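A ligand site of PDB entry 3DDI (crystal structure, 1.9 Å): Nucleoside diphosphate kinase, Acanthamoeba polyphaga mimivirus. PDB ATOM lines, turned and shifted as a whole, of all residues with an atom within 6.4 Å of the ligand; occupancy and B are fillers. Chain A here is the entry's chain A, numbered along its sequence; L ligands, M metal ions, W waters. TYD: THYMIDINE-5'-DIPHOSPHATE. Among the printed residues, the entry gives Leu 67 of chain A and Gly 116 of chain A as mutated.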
ATOM      1  N   LYS A  14      20.365  28.265   4.144  1.00  0.00           N
ATOM      2  CA  LYS A  14      19.444  27.404   3.405  1.00  0.00           C
ATOM      3  C   LYS A  14      19.465  27.716   1.906  1.00  0.00           C
ATOM      4  O   LYS A  14      19.977  28.758   1.497  1.00  0.00           O
ATOM      5  CB  LYS A  14      18.033  27.519   3.991  1.00  0.00           C
ATOM      6  CG  LYS A  14      17.943  27.031   5.429  1.00  0.00           C
ATOM      7  CD  LYS A  14      16.549  27.245   6.000  1.00  0.00           C
ATOM      8  CE  LYS A  14      16.399  26.529   7.345  1.00  0.00           C
ATOM      9  NZ  LYS A  14      15.051  26.774   7.949  1.00  0.00           N
ATOM     10  N   TYR A  55      15.865  17.466  11.058  1.00  0.00           N
ATOM     11  CA  TYR A  55      14.502  17.855  11.390  1.00  0.00           C
ATOM     12  C   TYR A  55      13.657  16.716  11.972  1.00  0.00           C
ATOM     13  O   TYR A  55      12.433  16.734  11.893  1.00  0.00           O
ATOM     14  CB  TYR A  55      13.822  18.439  10.145  1.00  0.00           C
ATOM     15  CG  TYR A  55      14.296  19.841   9.804  1.00  0.00           C
ATOM     16  CD1 TYR A  55      14.795  20.151   8.552  1.00  0.00           C
ATOM     17  CD2 TYR A  55      14.242  20.859  10.763  1.00  0.00           C
ATOM     18  CE1 TYR A  55      15.222  21.451   8.239  1.00  0.00           C
ATOM     19  CE2 TYR A  55      14.663  22.157  10.457  1.00  0.00           C
ATOM     20  CZ  TYR A  55      15.148  22.437   9.201  1.00  0.00           C
ATOM     21  OH  TYR A  55      15.577  23.714   8.897  1.00  0.00           O
ATOM     22  N   GLU A  57      12.575  16.037  14.749  1.00  0.00           N
ATOM     23  CA  GLU A  57      11.540  16.493  15.672  1.00  0.00           C
ATOM     24  C   GLU A  57      10.258  16.887  14.937  1.00  0.00           C
ATOM     25  O   GLU A  57       9.187  16.978  15.541  1.00  0.00           O
ATOM     26  CB  GLU A  57      12.056  17.663  16.527  1.00  0.00           C
ATOM     27  CG  GLU A  57      13.326  17.354  17.325  1.00  0.00           C
ATOM     28  CD  GLU A  57      14.089  18.606  17.782  1.00  0.00           C
ATOM     29  OE1 GLU A  57      14.285  18.774  19.006  1.00  0.00           O
ATOM     30  OE2 GLU A  57      14.496  19.426  16.923  1.00  0.00           O
ATOM     31  N   HIS A  58      10.369  17.111  13.629  1.00  0.00           N
ATOM     32  CA  HIS A  58       9.250  17.608  12.831  1.00  0.00           C
ATOM     33  C   HIS A  58       8.649  16.530  11.939  1.00  0.00           C
ATOM     34  O   HIS A  58       7.831  16.833  11.084  1.00  0.00           O
ATOM     35  CB  HIS A  58       9.726  18.764  11.950  1.00  0.00           C
ATOM     36  CG  HIS A  58      10.320  19.899  12.716  1.00  0.00           C
ATOM     37  ND1 HIS A  58       9.673  21.092  12.903  1.00  0.00           N
ATOM     38  CD2 HIS A  58      11.510  20.005  13.358  1.00  0.00           C
ATOM     39  CE1 HIS A  58      10.427  21.903  13.622  1.00  0.00           C
ATOM     40  NE2 HIS A  58      11.553  21.271  13.912  1.00  0.00           N
ATOM     41  N   TYR A  63       4.141  19.701   7.238  1.00  0.00           N
ATOM     42  CA  TYR A  63       5.070  20.379   6.336  1.00  0.00           C
ATOM     43  C   TYR A  63       6.388  19.626   6.172  1.00  0.00           C
ATOM     44  O   TYR A  63       7.246  20.054   5.418  1.00  0.00           O
ATOM     45  CB  TYR A  63       5.355  21.809   6.828  1.00  0.00           C
ATOM     46  CG  TYR A  63       5.900  21.901   8.226  1.00  0.00           C
ATOM     47  CD1 TYR A  63       7.213  21.542   8.501  1.00  0.00           C
ATOM     48  CD2 TYR A  63       5.099  22.339   9.278  1.00  0.00           C
ATOM     49  CE1 TYR A  63       7.720  21.620   9.781  1.00  0.00           C
ATOM     50  CE2 TYR A  63       5.606  22.408  10.570  1.00  0.00           C
ATOM     51  CZ  TYR A  63       6.911  22.052  10.811  1.00  0.00           C
ATOM     52  OH  TYR A  63       7.436  22.118  12.092  1.00  0.00           O
ATOM     53  N   LEU A  67       9.268  20.621   3.604  1.00  0.00           N
ATOM     54  CA  LEU A  67      10.467  21.139   4.246  1.00  0.00           C
ATOM     55  C   LEU A  67      11.717  20.414   3.749  1.00  0.00           C
ATOM     56  O   LEU A  67      12.718  21.040   3.392  1.00  0.00           O
ATOM     57  CB  LEU A  67      10.341  20.989   5.761  1.00  0.00           C
ATOM     58  CG  LEU A  67      11.618  21.241   6.565  1.00  0.00           C
ATOM     59  CD1 LEU A  67      12.125  22.674   6.379  1.00  0.00           C
ATOM     60  CD2 LEU A  67      11.350  20.935   8.014  1.00  0.00           C
ATOM     61  N   ARG A  91      20.167  32.963  17.698  1.00  0.00           N
ATOM     62  CA  ARG A  91      18.712  32.823  17.570  1.00  0.00           C
ATOM     63  C   ARG A  91      18.027  34.183  17.511  1.00  0.00           C
ATOM     64  O   ARG A  91      17.103  34.383  16.729  1.00  0.00           O
ATOM     65  CB  ARG A  91      18.139  32.002  18.729  1.00  0.00           C
ATOM     66  CG  ARG A  91      18.419  30.509  18.625  1.00  0.00           C
ATOM     67  CD  ARG A  91      17.476  29.864  17.597  1.00  0.00           C
ATOM     68  NE  ARG A  91      16.155  29.543  18.156  1.00  0.00           N
ATOM     69  CZ  ARG A  91      15.141  29.062  17.428  1.00  0.00           C
ATOM     70  NH1 ARG A  91      15.280  28.857  16.134  1.00  0.00           N
ATOM     71  NH2 ARG A  91      13.989  28.778  18.006  1.00  0.00           N
ATOM     72  N   GLN A  94      18.646  35.752  14.216  1.00  0.00           N
ATOM     73  CA  GLN A  94      17.864  35.004  13.235  1.00  0.00           C
ATOM     74  C   GLN A  94      16.461  35.577  13.042  1.00  0.00           C
ATOM     75  O   GLN A  94      16.029  35.832  11.905  1.00  0.00           O
ATOM     76  CB  GLN A  94      17.766  33.543  13.684  1.00  0.00           C
ATOM     77  CG  GLN A  94      16.958  32.648  12.752  1.00  0.00           C
ATOM     78  CD  GLN A  94      16.755  31.238  13.310  1.00  0.00           C
ATOM     79  OE1 GLN A  94      16.782  30.248  12.575  1.00  0.00           O
ATOM     80  NE2 GLN A  94      16.520  31.147  14.613  1.00  0.00           N
ATOM     81  N   GLY A  95      15.746  35.778  14.137  1.00  0.00           N
ATOM     82  CA  GLY A  95      14.381  36.252  14.046  1.00  0.00           C
ATOM     83  C   GLY A  95      13.393  35.111  14.025  1.00  0.00           C
ATOM     84  O   GLY A  95      13.744  33.971  13.691  1.00  0.00           O
ATOM     85  N   ASN A  96      12.153  35.401  14.372  1.00  0.00           N
ATOM     86  CA  ASN A  96      11.103  34.382  14.460  1.00  0.00           C
ATOM     87  C   ASN A  96      10.807  33.687  13.131  1.00  0.00           C
ATOM     88  O   ASN A  96      10.954  34.291  12.064  1.00  0.00           O
ATOM     89  CB  ASN A  96       9.821  34.994  15.022  1.00  0.00           C
ATOM     90  CG  ASN A  96       8.784  33.949  15.356  1.00  0.00           C
ATOM     91  OD1 ASN A  96       7.796  33.786  14.646  1.00  0.00           O
ATOM     92  ND2 ASN A  96       9.018  33.205  16.434  1.00  0.00           N
ATOM     93  N   THR A  97      10.371  32.429  13.193  1.00  0.00           N
ATOM     94  CA  THR A  97      10.030  31.645  12.018  1.00  0.00           C
ATOM     95  C   THR A  97       8.914  32.293  11.219  1.00  0.00           C
ATOM     96  O   THR A  97       8.914  32.291   9.988  1.00  0.00           O
ATOM     97  CB  THR A  97       9.509  30.243  12.413  1.00  0.00           C
ATOM     98  OG1 THR A  97      10.144  29.816  13.616  1.00  0.00           O
ATOM     99  CG2 THR A  97       9.770  29.236  11.312  1.00  0.00           C
ATOM    100  N   ASN A  98       7.946  32.846  11.941  1.00  0.00           N
ATOM    101  CA  ASN A  98       6.737  33.354  11.310  1.00  0.00           C
ATOM    102  C   ASN A  98       6.947  34.775  10.787  1.00  0.00           C
ATOM    103  O   ASN A  98       7.280  35.678  11.554  1.00  0.00           O
ATOM    104  CB  ASN A  98       5.577  33.321  12.316  1.00  0.00           C
ATOM    105  CG  ASN A  98       4.233  33.469  11.644  1.00  0.00           C
ATOM    106  OD1 ASN A  98       4.044  34.332  10.779  1.00  0.00           O
ATOM    107  ND2 ASN A  98       3.277  32.617  12.026  1.00  0.00           N
ATOM    108  N   ARG A 108      15.559  37.179   9.351  1.00  0.00           N
ATOM    109  CA  ARG A 108      14.267  36.880   8.750  1.00  0.00           C
ATOM    110  C   ARG A 108      13.368  38.120   8.653  1.00  0.00           C
ATOM    111  O   ARG A 108      12.626  38.296   7.685  1.00  0.00           O
ATOM    112  CB  ARG A 108      13.560  35.807   9.560  1.00  0.00           C
ATOM    113  CG  ARG A 108      14.201  34.432   9.378  1.00  0.00           C
ATOM    114  CD  ARG A 108      13.853  33.499  10.488  1.00  0.00           C
ATOM    115  NE  ARG A 108      14.245  32.125  10.174  1.00  0.00           N
ATOM    116  CZ  ARG A 108      14.009  31.086  10.966  1.00  0.00           C
ATOM    117  NH1 ARG A 108      13.435  31.262  12.149  1.00  0.00           N
ATOM    118  NH2 ARG A 108      14.380  29.876  10.580  1.00  0.00           N
ATOM    119  N   ASP A 114       8.580  34.157   4.038  1.00  0.00           N
ATOM    120  CA  ASP A 114       7.850  32.906   4.050  1.00  0.00           C
ATOM    121  C   ASP A 114       8.197  32.135   5.312  1.00  0.00           C
ATOM    122  O   ASP A 114       9.303  32.266   5.821  1.00  0.00           O
ATOM    123  CB  ASP A 114       8.217  32.078   2.828  1.00  0.00           C
ATOM    124  CG  ASP A 114       7.376  30.849   2.697  1.00  0.00           C
ATOM    125  OD1 ASP A 114       7.915  29.735   2.878  1.00  0.00           O
ATOM    126  OD2 ASP A 114       6.161  31.000   2.416  1.00  0.00           O
ATOM    127  N   ILE A 115       7.254  31.350   5.815  1.00  0.00           N
ATOM    128  CA  ILE A 115       7.504  30.585   7.037  1.00  0.00           C
ATOM    129  C   ILE A 115       8.424  29.391   6.762  1.00  0.00           C
ATOM    130  O   ILE A 115       9.114  28.928   7.655  1.00  0.00           O
ATOM    131  CB  ILE A 115       6.197  30.107   7.717  1.00  0.00           C
ATOM    132  CG1 ILE A 115       6.524  29.495   9.080  1.00  0.00           C
ATOM    133  CG2 ILE A 115       5.444  29.131   6.812  1.00  0.00           C
ATOM    134  CD1 ILE A 115       5.481  29.759  10.151  1.00  0.00           C
ATOM    135  N   GLY A 116       8.437  28.903   5.519  1.00  0.00           N
ATOM    136  CA  GLY A 116       9.298  27.782   5.157  1.00  0.00           C
ATOM    137  C   GLY A 116      10.618  28.230   4.561  1.00  0.00           C
ATOM    138  O   GLY A 116      11.688  27.802   5.012  1.00  0.00           O
ATOM    139  N   GLU A 117      10.556  29.085   3.549  1.00  0.00           N
ATOM    140  CA  GLU A 117      11.765  29.627   2.935  1.00  0.00           C
ATOM    141  C   GLU A 117      12.222  30.820   3.771  1.00  0.00           C
ATOM    142  O   GLU A 117      11.861  31.969   3.511  1.00  0.00           O
ATOM    143  CB  GLU A 117      11.520  29.975   1.471  1.00  0.00           C
ATOM    144  CG  GLU A 117      11.099  28.756   0.659  1.00  0.00           C
ATOM    145  CD  GLU A 117      10.830  29.065  -0.808  1.00  0.00           C
ATOM    146  OE1 GLU A 117      10.506  28.126  -1.551  1.00  0.00           O
ATOM    147  OE2 GLU A 117      10.945  30.245  -1.230  1.00  0.00           O
ATOM    148  N   ASN A 118      13.000  30.513   4.791  1.00  0.00           N
ATOM    149  CA  ASN A 118      13.338  31.497   5.797  1.00  0.00           C
ATOM    150  C   ASN A 118      14.844  31.636   5.995  1.00  0.00           C
ATOM    151  O   ASN A 118      15.285  32.023   7.066  1.00  0.00           O
ATOM    152  CB  ASN A 118      12.626  31.156   7.113  1.00  0.00           C
ATOM    153  CG  ASN A 118      13.017  29.785   7.641  1.00  0.00           C
ATOM    154  OD1 ASN A 118      14.170  29.371   7.510  1.00  0.00           O
ATOM    155  ND2 ASN A 118      12.060  29.073   8.243  1.00  0.00           N
ATOM    156  N   ILE A 120      17.724  30.662   7.034  1.00  0.00           N
ATOM    157  CA  ILE A 120      18.732  30.294   8.008  1.00  0.00           C
ATOM    158  C   ILE A 120      18.171  29.416   9.124  1.00  0.00           C
ATOM    159  O   ILE A 120      17.061  29.637   9.605  1.00  0.00           O
ATOM    160  CB  ILE A 120      19.391  31.568   8.649  1.00  0.00           C
ATOM    161  CG1 ILE A 120      20.403  31.174   9.728  1.00  0.00           C
ATOM    162  CG2 ILE A 120      18.327  32.504   9.234  1.00  0.00           C
ATOM    163  CD1 ILE A 120      21.266  32.341  10.237  1.00  0.00           C
ATOM    164  N   HIS A 121      18.934  28.404   9.507  1.00  0.00           N
ATOM    165  CA  HIS A 121      18.651  27.648  10.716  1.00  0.00           C
ATOM    166  C   HIS A 121      19.690  27.986  11.779  1.00  0.00           C
ATOM    167  O   HIS A 121      20.859  28.165  11.457  1.00  0.00           O
ATOM    168  CB  HIS A 121      18.721  26.158  10.445  1.00  0.00           C
ATOM    169  CG  HIS A 121      18.725  25.324  11.694  1.00  0.00           C
ATOM    170  ND1 HIS A 121      17.565  24.846  12.259  1.00  0.00           N
ATOM    171  CD2 HIS A 121      19.735  24.913  12.485  1.00  0.00           C
ATOM    172  CE1 HIS A 121      17.863  24.173  13.356  1.00  0.00           C
ATOM    173  NE2 HIS A 121      19.173  24.194  13.518  1.00  0.00           N
ATOM    174  N   ALA A 122      19.263  28.060  13.036  1.00  0.00           N
ATOM    175  CA  ALA A 122      20.168  28.162  14.169  1.00  0.00           C
ATOM    176  C   ALA A 122      19.660  27.268  15.299  1.00  0.00           C
ATOM    177  O   ALA A 122      18.463  27.248  15.581  1.00  0.00           O
ATOM    178  CB  ALA A 122      20.299  29.607  14.654  1.00  0.00           C
ATOM    179  N   ASP A 124      18.371  25.793  18.671  1.00  0.00           N
ATOM    180  CA  ASP A 124      17.530  26.525  19.625  1.00  0.00           C
ATOM    181  C   ASP A 124      17.890  26.321  21.101  1.00  0.00           C
ATOM    182  O   ASP A 124      17.351  27.006  21.968  1.00  0.00           O
ATOM    183  CB  ASP A 124      16.033  26.263  19.379  1.00  0.00           C
ATOM    184  CG  ASP A 124      15.632  24.809  19.638  1.00  0.00           C
ATOM    185  OD1 ASP A 124      16.482  24.019  20.082  1.00  0.00           O
ATOM    186  OD2 ASP A 124      14.450  24.471  19.389  1.00  0.00           O
HETATM  187  PA  TYD L   1      10.957  25.416  13.699  1.00  0.00           P
HETATM  188  O1A TYD L   1      12.072  24.678  14.396  1.00  0.00           O
HETATM  189  O2A TYD L   1       9.623  25.617  14.386  1.00  0.00           O
HETATM  190  O3A TYD L   1      11.451  26.864  13.171  1.00  0.00           O
HETATM  191  PB  TYD L   1      12.858  27.615  13.430  1.00  0.00           P
HETATM  192  O1B TYD L   1      13.635  27.334  12.169  1.00  0.00           O
HETATM  193  O2B TYD L   1      13.459  27.005  14.681  1.00  0.00           O
HETATM  194  O3B TYD L   1      12.438  29.061  13.579  1.00  0.00           O
HETATM  195  O5' TYD L   1      10.654  24.708  12.281  1.00  0.00           O
HETATM  196  C5' TYD L   1      11.712  24.138  11.511  1.00  0.00           C
HETATM  197  C4' TYD L   1      11.479  24.481  10.044  1.00  0.00           C
HETATM  198  O4' TYD L   1      10.257  23.910   9.584  1.00  0.00           O
HETATM  199  C3' TYD L   1      11.328  25.975   9.804  1.00  0.00           C
HETATM  200  O3' TYD L   1      12.595  26.626   9.626  1.00  0.00           O
HETATM  201  C2' TYD L   1      10.490  26.042   8.542  1.00  0.00           C
HETATM  202  C1' TYD L   1       9.658  24.769   8.609  1.00  0.00           C
HETATM  203  N1  TYD L   1       8.303  25.114   9.031  1.00  0.00           N
HETATM  204  C2  TYD L   1       7.293  25.238   8.050  1.00  0.00           C
HETATM  205  O2  TYD L   1       7.573  25.051   6.840  1.00  0.00           O
HETATM  206  N3  TYD L   1       6.049  25.556   8.400  1.00  0.00           N
HETATM  207  C4  TYD L   1       5.721  25.749   9.676  1.00  0.00           C
HETATM  208  O4  TYD L   1       4.543  26.046   9.984  1.00  0.00           O
HETATM  209  C5  TYD L   1       6.769  25.630  10.731  1.00  0.00           C
HETATM  210  C5M TYD L   1       6.460  25.841  12.190  1.00  0.00           C
HETATM  211  C6  TYD L   1       8.056  25.294  10.333  1.00  0.00           C
HETATM  212 MG    MG M   1      14.406  24.793  15.791  1.00  0.00          MG
HETATM  213  O   HOH W   1       4.002  25.437   6.781  1.00  0.00           O
HETATM  214  O   HOH W   2      14.314  22.429  14.651  1.00  0.00           O
HETATM  215  O   HOH W   3      15.354  25.757  10.733  1.00  0.00           O
HETATM  216  O   HOH W   4      16.247  27.533  13.487  1.00  0.00           O
HETATM  217  O   HOH W   5      12.166  30.846  15.539  1.00  0.00           O
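Tyr 55 touches the ligand (CE2 to C5', 3.7 Å). Tyr 63 touches the ligand (CE1 to O4', 3.4 Å). CD2 of Leu 67 touches O4' of the ligand, 3.5 Å away. Ile 115 touches the ligand. Gly 116 touches the ligand (CA to O2, 3.6 Å). Hydrophobic or aromatic side chains that line the ligand: Tyr 55, His 58, Tyr 63, Leu 67 and Ile 115. The nearest printed residue that does not touch the ligand is Gln 94 (4.3 Å).
The guanidinium group of Arg 91 is in salt-bridge range of an oxygen (O2B) of the ligand, at 3.0 Å. O1A of the ligand sits close to NE2 of His 58. O3' of the ligand lies within hydrogen-bond range of ND2 of Asn 118 (2.9 Å). An oxygen (O3') of the ligand sits at hydrogen-bond distance from the side-chain amino group (NZ) of Lys 14 (3.0 Å). The side-chain hydroxyl (OG1) of Thr 97 sits at hydrogen-bond distance from an oxygen (O3B) of the ligand (2.4 Å). The guanidinium group (NH1) of Arg 108 lies within salt-bridge range of an oxygen (O3B) of the ligand, 2.8 Å away.
Water W5 lies within hydrogen-bond range of an oxygen (O3B) of the ligand (2.7 Å) and the side-chain hydroxyl (OG1) of Thr 97 (3.0 Å). Water W3 lies within hydrogen-bond range of an oxygen (O1B) of the ligand (2.7 Å), the side-chain hydroxyl (OH) of Tyr 55 (2.8 Å), a ring nitrogen (ND1) of His 121 (2.8 Å) and the side-chain amino group (NZ) of Lys 14 (3.0 Å). Water W4 lies within hydrogen-bond range of OE1 of Gln 94 (2.9 Å), O1B of the ligand (2.9 Å), O of Ala 122 (3.1 Å), NH1 of Arg 91 (3.1 Å) and ND1 of His 121 (3.2 Å). Water W2 bridges NE2 of His 58 (3.1 Å) and O1A of the ligand (3.2 Å).
The side-chain amide nitrogen (ND2) of Asn 118 lies within hydrogen-bond range of the backbone carbonyl oxygen (O) of Ile 115 (3.0 Å). NE2 of Gln 94 lies close to NH1 of Arg 91 (3.0 Å). NZ of Lys 14 lies within hydrogen-bond range of OD1 of Asn 118 (2.8 Å). A ring nitrogen (ND1) of His 58 lies within hydrogen-bond range of the side-chain hydroxyl (OH) of Tyr 63, at 2.6 Å. The side-chain hydroxyl (OH) of Tyr 55 sits at hydrogen-bond distance from the side-chain amino group (NZ) of Lys 14, at 3.2 Å. The backbone NH of Gly 116 sits at hydrogen-bond distance from the side-chain carboxylate of Asp 114 (2.8 Å). N of Arg 108 is in hydrogen-bond range of O of Gln 94, 2.9 Å away. The side-chain amide oxygen (OD1) of Asn 118 is in hydrogen-bond range of the guanidinium group (NH2) of Arg 108, at 3.1 Å.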
